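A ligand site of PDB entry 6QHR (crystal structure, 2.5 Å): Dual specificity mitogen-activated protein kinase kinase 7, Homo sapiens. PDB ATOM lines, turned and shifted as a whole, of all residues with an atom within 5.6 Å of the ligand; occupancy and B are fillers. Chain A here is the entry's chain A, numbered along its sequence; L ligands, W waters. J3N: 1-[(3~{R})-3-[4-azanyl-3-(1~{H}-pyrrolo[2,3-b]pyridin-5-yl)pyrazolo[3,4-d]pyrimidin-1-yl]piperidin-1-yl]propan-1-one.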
ATOM      1  N   MET A  36     -15.289  21.769  10.355  1.00  0.00           N
ATOM      2  CA  MET A  36     -16.590  22.300  10.697  1.00  0.00           C
ATOM      3  C   MET A  36     -17.627  21.242  10.341  1.00  0.00           C
ATOM      4  O   MET A  36     -17.922  21.027   9.159  1.00  0.00           O
ATOM      5  CB  MET A  36     -16.843  23.634   9.992  1.00  0.00           C
ATOM      6  CG  MET A  36     -15.839  24.696  10.412  1.00  0.00           C
ATOM      7  SD  MET A  36     -16.023  26.311   9.639  1.00  0.00           S
ATOM      8  CE  MET A  36     -14.671  26.289   8.483  1.00  0.00           C
ATOM      9  N   GLY A  37     -18.165  20.581  11.353  1.00  0.00           N
ATOM     10  CA  GLY A  37     -18.858  19.310  11.192  1.00  0.00           C
ATOM     11  C   GLY A  37     -20.149  19.314  10.413  1.00  0.00           C
ATOM     12  O   GLY A  37     -21.204  19.712  10.939  1.00  0.00           O
ATOM     13  N   SER A  38     -20.084  18.853   9.162  1.00  0.00           N
ATOM     14  CA  SER A  38     -21.198  18.489   8.296  1.00  0.00           C
ATOM     15  C   SER A  38     -20.642  18.196   6.907  1.00  0.00           C
ATOM     16  O   SER A  38     -19.524  18.587   6.578  1.00  0.00           O
ATOM     17  CB  SER A  38     -22.288  19.564   8.206  1.00  0.00           C
ATOM     18  N   THR A  40     -22.676  18.834   3.899  1.00  0.00           N
ATOM     19  CA  THR A  40     -23.750  19.299   3.026  1.00  0.00           C
ATOM     20  C   THR A  40     -23.326  19.218   1.556  1.00  0.00           C
ATOM     21  O   THR A  40     -24.067  18.693   0.715  1.00  0.00           O
ATOM     22  CB  THR A  40     -24.137  20.737   3.382  1.00  0.00           C
ATOM     23  N   VAL A  44     -15.408  20.643   4.923  1.00  0.00           N
ATOM     24  CA  VAL A  44     -15.062  22.050   5.132  1.00  0.00           C
ATOM     25  C   VAL A  44     -14.139  22.142   6.338  1.00  0.00           C
ATOM     26  O   VAL A  44     -14.492  21.736   7.451  1.00  0.00           O
ATOM     27  CB  VAL A  44     -16.313  22.926   5.348  1.00  0.00           C
ATOM     28  CG1 VAL A  44     -15.902  24.357   5.579  1.00  0.00           C
ATOM     29  CG2 VAL A  44     -17.237  22.835   4.142  1.00  0.00           C
ATOM     30  N   ALA A  57     -12.066  29.572   5.832  1.00  0.00           N
ATOM     31  CA  ALA A  57     -12.722  28.301   5.579  1.00  0.00           C
ATOM     32  C   ALA A  57     -12.270  27.751   4.230  1.00  0.00           C
ATOM     33  O   ALA A  57     -12.279  28.475   3.229  1.00  0.00           O
ATOM     34  CB  ALA A  57     -14.249  28.462   5.588  1.00  0.00           C
ATOM     35  N   VAL A  58     -11.871  26.475   4.225  1.00  0.00           N
ATOM     36  CA  VAL A  58     -11.387  25.812   3.020  1.00  0.00           C
ATOM     37  C   VAL A  58     -12.146  24.503   2.840  1.00  0.00           C
ATOM     38  O   VAL A  58     -12.218  23.690   3.763  1.00  0.00           O
ATOM     39  CB  VAL A  58      -9.866  25.540   3.082  1.00  0.00           C
ATOM     40  CG1 VAL A  58      -9.355  25.027   1.746  1.00  0.00           C
ATOM     41  CG2 VAL A  58      -9.122  26.797   3.524  1.00  0.00           C
ATOM     42  N   LYS A  59     -12.719  24.315   1.653  1.00  0.00           N
ATOM     43  CA  LYS A  59     -13.407  23.077   1.293  1.00  0.00           C
ATOM     44  C   LYS A  59     -12.481  22.207   0.474  1.00  0.00           C
ATOM     45  O   LYS A  59     -11.907  22.669  -0.525  1.00  0.00           O
ATOM     46  CB  LYS A  59     -14.685  23.380   0.500  1.00  0.00           C
ATOM     47  CG  LYS A  59     -15.403  22.137   0.009  1.00  0.00           C
ATOM     48  CD  LYS A  59     -16.569  22.462  -0.900  1.00  0.00           C
ATOM     49  CE  LYS A  59     -17.599  23.317  -0.189  1.00  0.00           C
ATOM     50  NZ  LYS A  59     -18.819  23.461  -1.030  1.00  0.00           N
ATOM     51  N   ASP A  76     -21.410  24.546  -7.292  1.00  0.00           N
ATOM     52  CA  ASP A  76     -21.457  25.593  -6.279  1.00  0.00           C
ATOM     53  C   ASP A  76     -20.346  26.621  -6.475  1.00  0.00           C
ATOM     54  O   ASP A  76     -20.573  27.824  -6.313  1.00  0.00           O
ATOM     55  CB  ASP A  76     -21.378  24.978  -4.888  1.00  0.00           C
ATOM     56  CG  ASP A  76     -21.094  26.000  -3.810  1.00  0.00           C
ATOM     57  OD1 ASP A  76     -22.009  26.795  -3.513  1.00  0.00           O
ATOM     58  OD2 ASP A  76     -19.963  26.010  -3.279  1.00  0.00           O
ATOM     59  N   VAL A  80     -20.450  30.813  -7.238  1.00  0.00           N
ATOM     60  CA  VAL A  80     -19.787  31.719  -6.300  1.00  0.00           C
ATOM     61  C   VAL A  80     -18.798  32.622  -7.034  1.00  0.00           C
ATOM     62  O   VAL A  80     -18.662  33.814  -6.721  1.00  0.00           O
ATOM     63  CB  VAL A  80     -19.110  30.922  -5.172  1.00  0.00           C
ATOM     64  CG1 VAL A  80     -18.171  31.814  -4.384  1.00  0.00           C
ATOM     65  CG2 VAL A  80     -20.159  30.319  -4.267  1.00  0.00           C
ATOM     66  N   VAL A  90     -21.914  34.602  -0.546  1.00  0.00           N
ATOM     67  CA  VAL A  90     -20.605  34.307   0.029  1.00  0.00           C
ATOM     68  C   VAL A  90     -19.517  34.426  -1.042  1.00  0.00           C
ATOM     69  O   VAL A  90     -19.734  34.124  -2.222  1.00  0.00           O
ATOM     70  CB  VAL A  90     -20.593  32.919   0.674  1.00  0.00           C
ATOM     71  CG1 VAL A  90     -21.439  32.910   1.925  1.00  0.00           C
ATOM     72  CG2 VAL A  90     -21.105  31.881  -0.312  1.00  0.00           C
ATOM     73  N   ILE A 104     -10.786  25.015  -1.948  1.00  0.00           N
ATOM     74  CA  ILE A 104     -11.563  26.210  -2.236  1.00  0.00           C
ATOM     75  C   ILE A 104     -11.572  27.072  -0.985  1.00  0.00           C
ATOM     76  O   ILE A 104     -12.194  26.713   0.025  1.00  0.00           O
ATOM     77  CB  ILE A 104     -13.001  25.856  -2.672  1.00  0.00           C
ATOM     78  CG1 ILE A 104     -12.980  24.840  -3.809  1.00  0.00           C
ATOM     79  CG2 ILE A 104     -13.752  27.104  -3.077  1.00  0.00           C
ATOM     80  CD1 ILE A 104     -14.350  24.363  -4.204  1.00  0.00           C
ATOM     81  N   ALA A 105     -10.879  28.210  -1.035  1.00  0.00           N
ATOM     82  CA  ALA A 105     -10.850  29.103   0.107  1.00  0.00           C
ATOM     83  C   ALA A 105     -12.069  30.006   0.091  1.00  0.00           C
ATOM     84  O   ALA A 105     -12.534  30.422  -0.971  1.00  0.00           O
ATOM     85  CB  ALA A 105      -9.568  29.942   0.098  1.00  0.00           C
ATOM     86  N   MET A 106     -12.598  30.296   1.280  1.00  0.00           N
ATOM     87  CA  MET A 106     -13.797  31.110   1.389  1.00  0.00           C
ATOM     88  C   MET A 106     -13.759  31.907   2.690  1.00  0.00           C
ATOM     89  O   MET A 106     -13.124  31.503   3.667  1.00  0.00           O
ATOM     90  CB  MET A 106     -15.065  30.260   1.324  1.00  0.00           C
ATOM     91  CG  MET A 106     -16.277  31.028   0.861  1.00  0.00           C
ATOM     92  SD  MET A 106     -17.687  29.996   0.397  1.00  0.00           S
ATOM     93  CE  MET A 106     -18.752  30.204   1.814  1.00  0.00           C
ATOM     94  N   GLU A 107     -14.451  33.045   2.688  1.00  0.00           N
ATOM     95  CA  GLU A 107     -14.578  33.839   3.902  1.00  0.00           C
ATOM     96  C   GLU A 107     -15.256  33.021   4.993  1.00  0.00           C
ATOM     97  O   GLU A 107     -16.233  32.308   4.746  1.00  0.00           O
ATOM     98  CB  GLU A 107     -15.353  35.121   3.625  1.00  0.00           C
ATOM     99  CG  GLU A 107     -16.762  34.913   3.070  1.00  0.00           C
ATOM    100  CD  GLU A 107     -17.573  36.198   3.038  1.00  0.00           C
ATOM    101  OE1 GLU A 107     -17.274  37.112   3.838  1.00  0.00           O
ATOM    102  OE2 GLU A 107     -18.511  36.289   2.213  1.00  0.00           O
ATOM    103  N   LEU A 108     -14.725  33.129   6.210  1.00  0.00           N
ATOM    104  CA  LEU A 108     -15.255  32.363   7.333  1.00  0.00           C
ATOM    105  C   LEU A 108     -16.406  33.143   7.957  1.00  0.00           C
ATOM    106  O   LEU A 108     -16.209  34.207   8.560  1.00  0.00           O
ATOM    107  CB  LEU A 108     -14.147  32.084   8.345  1.00  0.00           C
ATOM    108  CG  LEU A 108     -14.488  31.181   9.530  1.00  0.00           C
ATOM    109  CD1 LEU A 108     -13.275  30.362   9.898  1.00  0.00           C
ATOM    110  CD2 LEU A 108     -14.927  32.012  10.715  1.00  0.00           C
ATOM    111  N   MET A 109     -17.617  32.608   7.816  1.00  0.00           N
ATOM    112  CA  MET A 109     -18.790  33.170   8.463  1.00  0.00           C
ATOM    113  C   MET A 109     -18.903  32.637   9.891  1.00  0.00           C
ATOM    114  O   MET A 109     -18.213  31.697  10.288  1.00  0.00           O
ATOM    115  CB  MET A 109     -20.056  32.841   7.660  1.00  0.00           C
ATOM    116  CG  MET A 109     -20.000  33.239   6.182  1.00  0.00           C
ATOM    117  SD  MET A 109     -20.091  35.029   5.899  1.00  0.00           S
ATOM    118  CE  MET A 109     -21.701  35.392   6.596  1.00  0.00           C
ATOM    119  N   GLY A 110     -19.804  33.234  10.665  1.00  0.00           N
ATOM    120  CA  GLY A 110     -20.004  32.794  12.032  1.00  0.00           C
ATOM    121  C   GLY A 110     -20.849  31.544  12.127  1.00  0.00           C
ATOM    122  O   GLY A 110     -20.339  30.465  12.430  1.00  0.00           O
ATOM    123  N   THR A 111     -22.150  31.679  11.862  1.00  0.00           N
ATOM    124  CA  THR A 111     -23.079  30.585  12.064  1.00  0.00           C
ATOM    125  C   THR A 111     -24.209  30.684  11.044  1.00  0.00           C
ATOM    126  O   THR A 111     -24.508  31.755  10.527  1.00  0.00           O
ATOM    127  CB  THR A 111     -23.658  30.590  13.487  1.00  0.00           C
ATOM    128  OG1 THR A 111     -22.655  31.016  14.419  1.00  0.00           O
ATOM    129  CG2 THR A 111     -24.112  29.213  13.870  1.00  0.00           C
ATOM    130  N   CYS A 112     -24.845  29.547  10.782  1.00  0.00           N
ATOM    131  CA  CYS A 112     -26.029  29.519   9.949  1.00  0.00           C
ATOM    132  C   CYS A 112     -27.272  29.798  10.792  1.00  0.00           C
ATOM    133  O   CYS A 112     -27.254  29.724  12.014  1.00  0.00           O
ATOM    134  CB  CYS A 112     -26.157  28.173   9.242  1.00  0.00           C
ATOM    135  SG  CYS A 112     -26.596  26.787  10.304  1.00  0.00           S
ATOM    136  N   ALA A 113     -28.365  30.149  10.103  1.00  0.00           N
ATOM    137  CA  ALA A 113     -29.580  30.536  10.820  1.00  0.00           C
ATOM    138  C   ALA A 113     -30.200  29.371  11.570  1.00  0.00           C
ATOM    139  O   ALA A 113     -30.918  29.583  12.561  1.00  0.00           O
ATOM    140  CB  ALA A 113     -30.586  31.142   9.848  1.00  0.00           C
ATOM    141  N   GLU A 114     -29.950  28.129  11.128  1.00  0.00           N
ATOM    142  CA  GLU A 114     -30.490  26.962  11.829  1.00  0.00           C
ATOM    143  C   GLU A 114     -29.856  26.806  13.207  1.00  0.00           C
ATOM    144  O   GLU A 114     -30.560  26.649  14.213  1.00  0.00           O
ATOM    145  CB  GLU A 114     -30.274  25.703  10.994  1.00  0.00           C
ATOM    146  CG  GLU A 114     -30.754  24.439  11.687  1.00  0.00           C
ATOM    147  CD  GLU A 114     -30.596  23.186  10.833  1.00  0.00           C
ATOM    148  OE1 GLU A 114     -31.034  22.104  11.277  1.00  0.00           O
ATOM    149  OE2 GLU A 114     -30.048  23.279   9.715  1.00  0.00           O
ATOM    150  N   LYS A 115     -28.523  26.853  13.269  1.00  0.00           N
ATOM    151  CA  LYS A 115     -27.838  26.755  14.561  1.00  0.00           C
ATOM    152  C   LYS A 115     -28.141  27.959  15.446  1.00  0.00           C
ATOM    153  O   LYS A 115     -28.124  27.829  16.677  1.00  0.00           O
ATOM    154  CB  LYS A 115     -26.336  26.606  14.352  1.00  0.00           C
ATOM    155  CG  LYS A 115     -25.810  25.177  14.436  1.00  0.00           C
ATOM    156  CD  LYS A 115     -26.396  24.290  13.359  1.00  0.00           C
ATOM    157  CE  LYS A 115     -25.619  22.988  13.279  1.00  0.00           C
ATOM    158  NZ  LYS A 115     -24.185  23.255  12.976  1.00  0.00           N
ATOM    159  N   SER A 157     -30.565  26.643   6.990  1.00  0.00           N
ATOM    160  CA  SER A 157     -29.193  26.169   7.069  1.00  0.00           C
ATOM    161  C   SER A 157     -28.302  26.739   5.974  1.00  0.00           C
ATOM    162  O   SER A 157     -27.078  26.575   6.049  1.00  0.00           O
ATOM    163  CB  SER A 157     -29.137  24.635   7.012  1.00  0.00           C
ATOM    164  OG  SER A 157     -29.656  24.139   5.788  1.00  0.00           O
ATOM    165  N   LEU A 160     -26.131  32.285   6.153  1.00  0.00           N
ATOM    166  CA  LEU A 160     -25.026  32.431   7.095  1.00  0.00           C
ATOM    167  C   LEU A 160     -24.977  33.843   7.663  1.00  0.00           C
ATOM    168  O   LEU A 160     -25.399  34.812   7.026  1.00  0.00           O
ATOM    169  CB  LEU A 160     -23.691  32.093   6.431  1.00  0.00           C
ATOM    170  CG  LEU A 160     -23.615  30.695   5.789  1.00  0.00           C
ATOM    171  CD1 LEU A 160     -22.267  30.443   5.128  1.00  0.00           C
ATOM    172  CD2 LEU A 160     -23.939  29.601   6.809  1.00  0.00           C
ATOM    173  N   CYS A 170     -25.652  31.025   0.720  1.00  0.00           N
ATOM    174  CA  CYS A 170     -24.582  30.100   0.346  1.00  0.00           C
ATOM    175  C   CYS A 170     -25.169  28.792  -0.174  1.00  0.00           C
ATOM    176  O   CYS A 170     -26.389  28.580  -0.174  1.00  0.00           O
ATOM    177  CB  CYS A 170     -23.635  29.835   1.520  1.00  0.00           C
ATOM    178  SG  CYS A 170     -24.182  28.491   2.609  1.00  0.00           S
ATOM    179  N   ASP A 171     -24.268  27.903  -0.613  1.00  0.00           N
ATOM    180  CA  ASP A 171     -24.553  26.544  -1.055  1.00  0.00           C
ATOM    181  C   ASP A 171     -25.442  26.504  -2.296  1.00  0.00           C
ATOM    182  O   ASP A 171     -26.671  26.419  -2.179  1.00  0.00           O
ATOM    183  CB  ASP A 171     -25.183  25.723   0.064  1.00  0.00           C
ATOM    184  CG  ASP A 171     -24.941  24.224  -0.106  1.00  0.00           C
ATOM    185  OD1 ASP A 171     -24.855  23.749  -1.256  1.00  0.00           O
ATOM    186  OD2 ASP A 171     -24.808  23.532   0.934  1.00  0.00           O
HETATM  187  C11 J3N L   1     -23.688  24.538   8.793  1.00  0.00           C
HETATM  188  C13 J3N L   1     -25.846  25.320   9.668  1.00  0.00           C
HETATM  189  C16 J3N L   1     -18.381  26.755   0.361  1.00  0.00           C
HETATM  190  C17 J3N L   1     -19.859  26.986   2.148  1.00  0.00           C
HETATM  191  C18 J3N L   1     -16.027  26.499   0.587  1.00  0.00           C
HETATM  192  C19 J3N L   1     -16.444  26.501  -0.735  1.00  0.00           C
HETATM  193  N   J3N L   1     -18.005  29.901   6.840  1.00  0.00           N
HETATM  194  C   J3N L   1     -18.587  29.405   7.940  1.00  0.00           C
HETATM  195  O   J3N L   1     -23.650  23.817   9.772  1.00  0.00           O
HETATM  196  C1  J3N L   1     -19.438  27.523   6.826  1.00  0.00           C
HETATM  197  C10 J3N L   1     -22.311  25.414   6.929  1.00  0.00           C
HETATM  198  C12 J3N L   1     -24.669  25.686   8.773  1.00  0.00           C
HETATM  199  C14 J3N L   1     -17.498  26.727   2.676  1.00  0.00           C
HETATM  200  C15 J3N L   1     -17.254  26.658   1.307  1.00  0.00           C
HETATM  201  C2  J3N L   1     -18.817  27.994   5.572  1.00  0.00           C
HETATM  202  C3  J3N L   1     -18.069  29.272   5.650  1.00  0.00           C
HETATM  203  C4  J3N L   1     -19.157  26.966   4.539  1.00  0.00           C
HETATM  204  C5  J3N L   1     -18.824  26.904   3.087  1.00  0.00           C
HETATM  205  C6  J3N L   1     -20.844  25.412   7.340  1.00  0.00           C
HETATM  206  C7  J3N L   1     -20.242  24.028   7.128  1.00  0.00           C
HETATM  207  C8  J3N L   1     -21.078  22.922   7.771  1.00  0.00           C
HETATM  208  C9  J3N L   1     -22.522  23.014   7.303  1.00  0.00           C
HETATM  209  N1  J3N L   1     -19.293  28.261   7.950  1.00  0.00           N
HETATM  210  N2  J3N L   1     -20.059  26.386   6.526  1.00  0.00           N
HETATM  211  N3  J3N L   1     -19.902  26.028   5.177  1.00  0.00           N
HETATM  212  N4  J3N L   1     -17.456  29.807   4.573  1.00  0.00           N
HETATM  213  N5  J3N L   1     -22.903  24.349   7.733  1.00  0.00           N
HETATM  214  N6  J3N L   1     -19.647  26.925   0.829  1.00  0.00           N
HETATM  215  N7  J3N L   1     -17.803  26.653  -0.856  1.00  0.00           N
HETATM  216  O   HOH W   1     -20.640  27.537  10.880  1.00  0.00           O
HETATM  217  O   HOH W   2     -17.796  24.796  -3.806  1.00  0.00           O
HETATM  218  O   HOH W   3     -21.115  28.173  -0.996  1.00  0.00           O
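Water W3 lies within hydrogen-bond range of N6 of the ligand (2.7 Å), OD1 of Asp 76 (3.0 Å) and N of Asp 171 (3.2 Å). Water W1 bridges N1 of the ligand (3.3 Å) and O of Gly 110 (3.3 Å). Water W2 lies within hydrogen-bond range of OD2 of Asp 76 (2.5 Å), NZ of Lys 59 (3.2 Å) and N7 of the ligand (3.5 Å).
N of Lys 115 sits at hydrogen-bond distance from SG of Cys 112 (3.5 Å). N of Glu 114 sits close to SG of Cys 112 (3.7 Å). O of Ala 57 sits at hydrogen-bond distance from N of Met 106 (2.7 Å). The side-chain carboxylate (OD2) of Asp 76 is in salt-bridge range of the side-chain amino group (NZ) of Lys 59 (3.6 Å). The backbone carbonyl oxygen (O) of Ile 104 lies within hydrogen-bond range of the backbone NH (N) of Lys 59, 2.9 Å away. The backbone NH (N) of Met 36 lies within hydrogen-bond range of the backbone carbonyl oxygen (O) of Val 44.
The side-chain sulfur of Cys 112 is covalently linked to a carbon (C13) of the ligand, at 1.8 Å. O of Glu 107 sits at hydrogen-bond distance from N4 of the ligand (2.8 Å). N of Met 109 lies within hydrogen-bond range of N of the ligand (2.9 Å). SD of Met 106 lies close to N7 of the ligand. The side-chain amino group of Lys 115 lies within hydrogen-bond range of an oxygen (O) of the ligand, 3.3 Å away. The side-chain carboxylate of Asp 76 sits at hydrogen-bond distance from a nitrogen (N7) of the ligand (3.3 Å). A nitrogen (N7) of the ligand lies close to the side-chain amino group (NZ) of Lys 59 (3.4 Å).
O of Met 36 touches C8 of the ligand, at 3.9 Å. Ser 38 touches the ligand (CB to C9, 3.6 Å). Ala 57 touches the ligand. CG2 of Ile 104 touches C19 of the ligand, 3.6 Å away. Leu 108 touches the ligand (CA to N, 3.7 Å). Ser 157 touches the ligand (O to C12, 3.7 Å). Hydrophobic or aromatic side chains that line the ligand: Ala 57, Ile 104, Met 106 and Met 109. 13 residues have an atom within 4 Å of the ligand: Met 36, Ser 38, Ala 57, Lys 59, Asp 76, Ile 104, Met 106, Glu 107, Leu 108, Met 109, Cys 112, Lys 115 and Ser 157.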
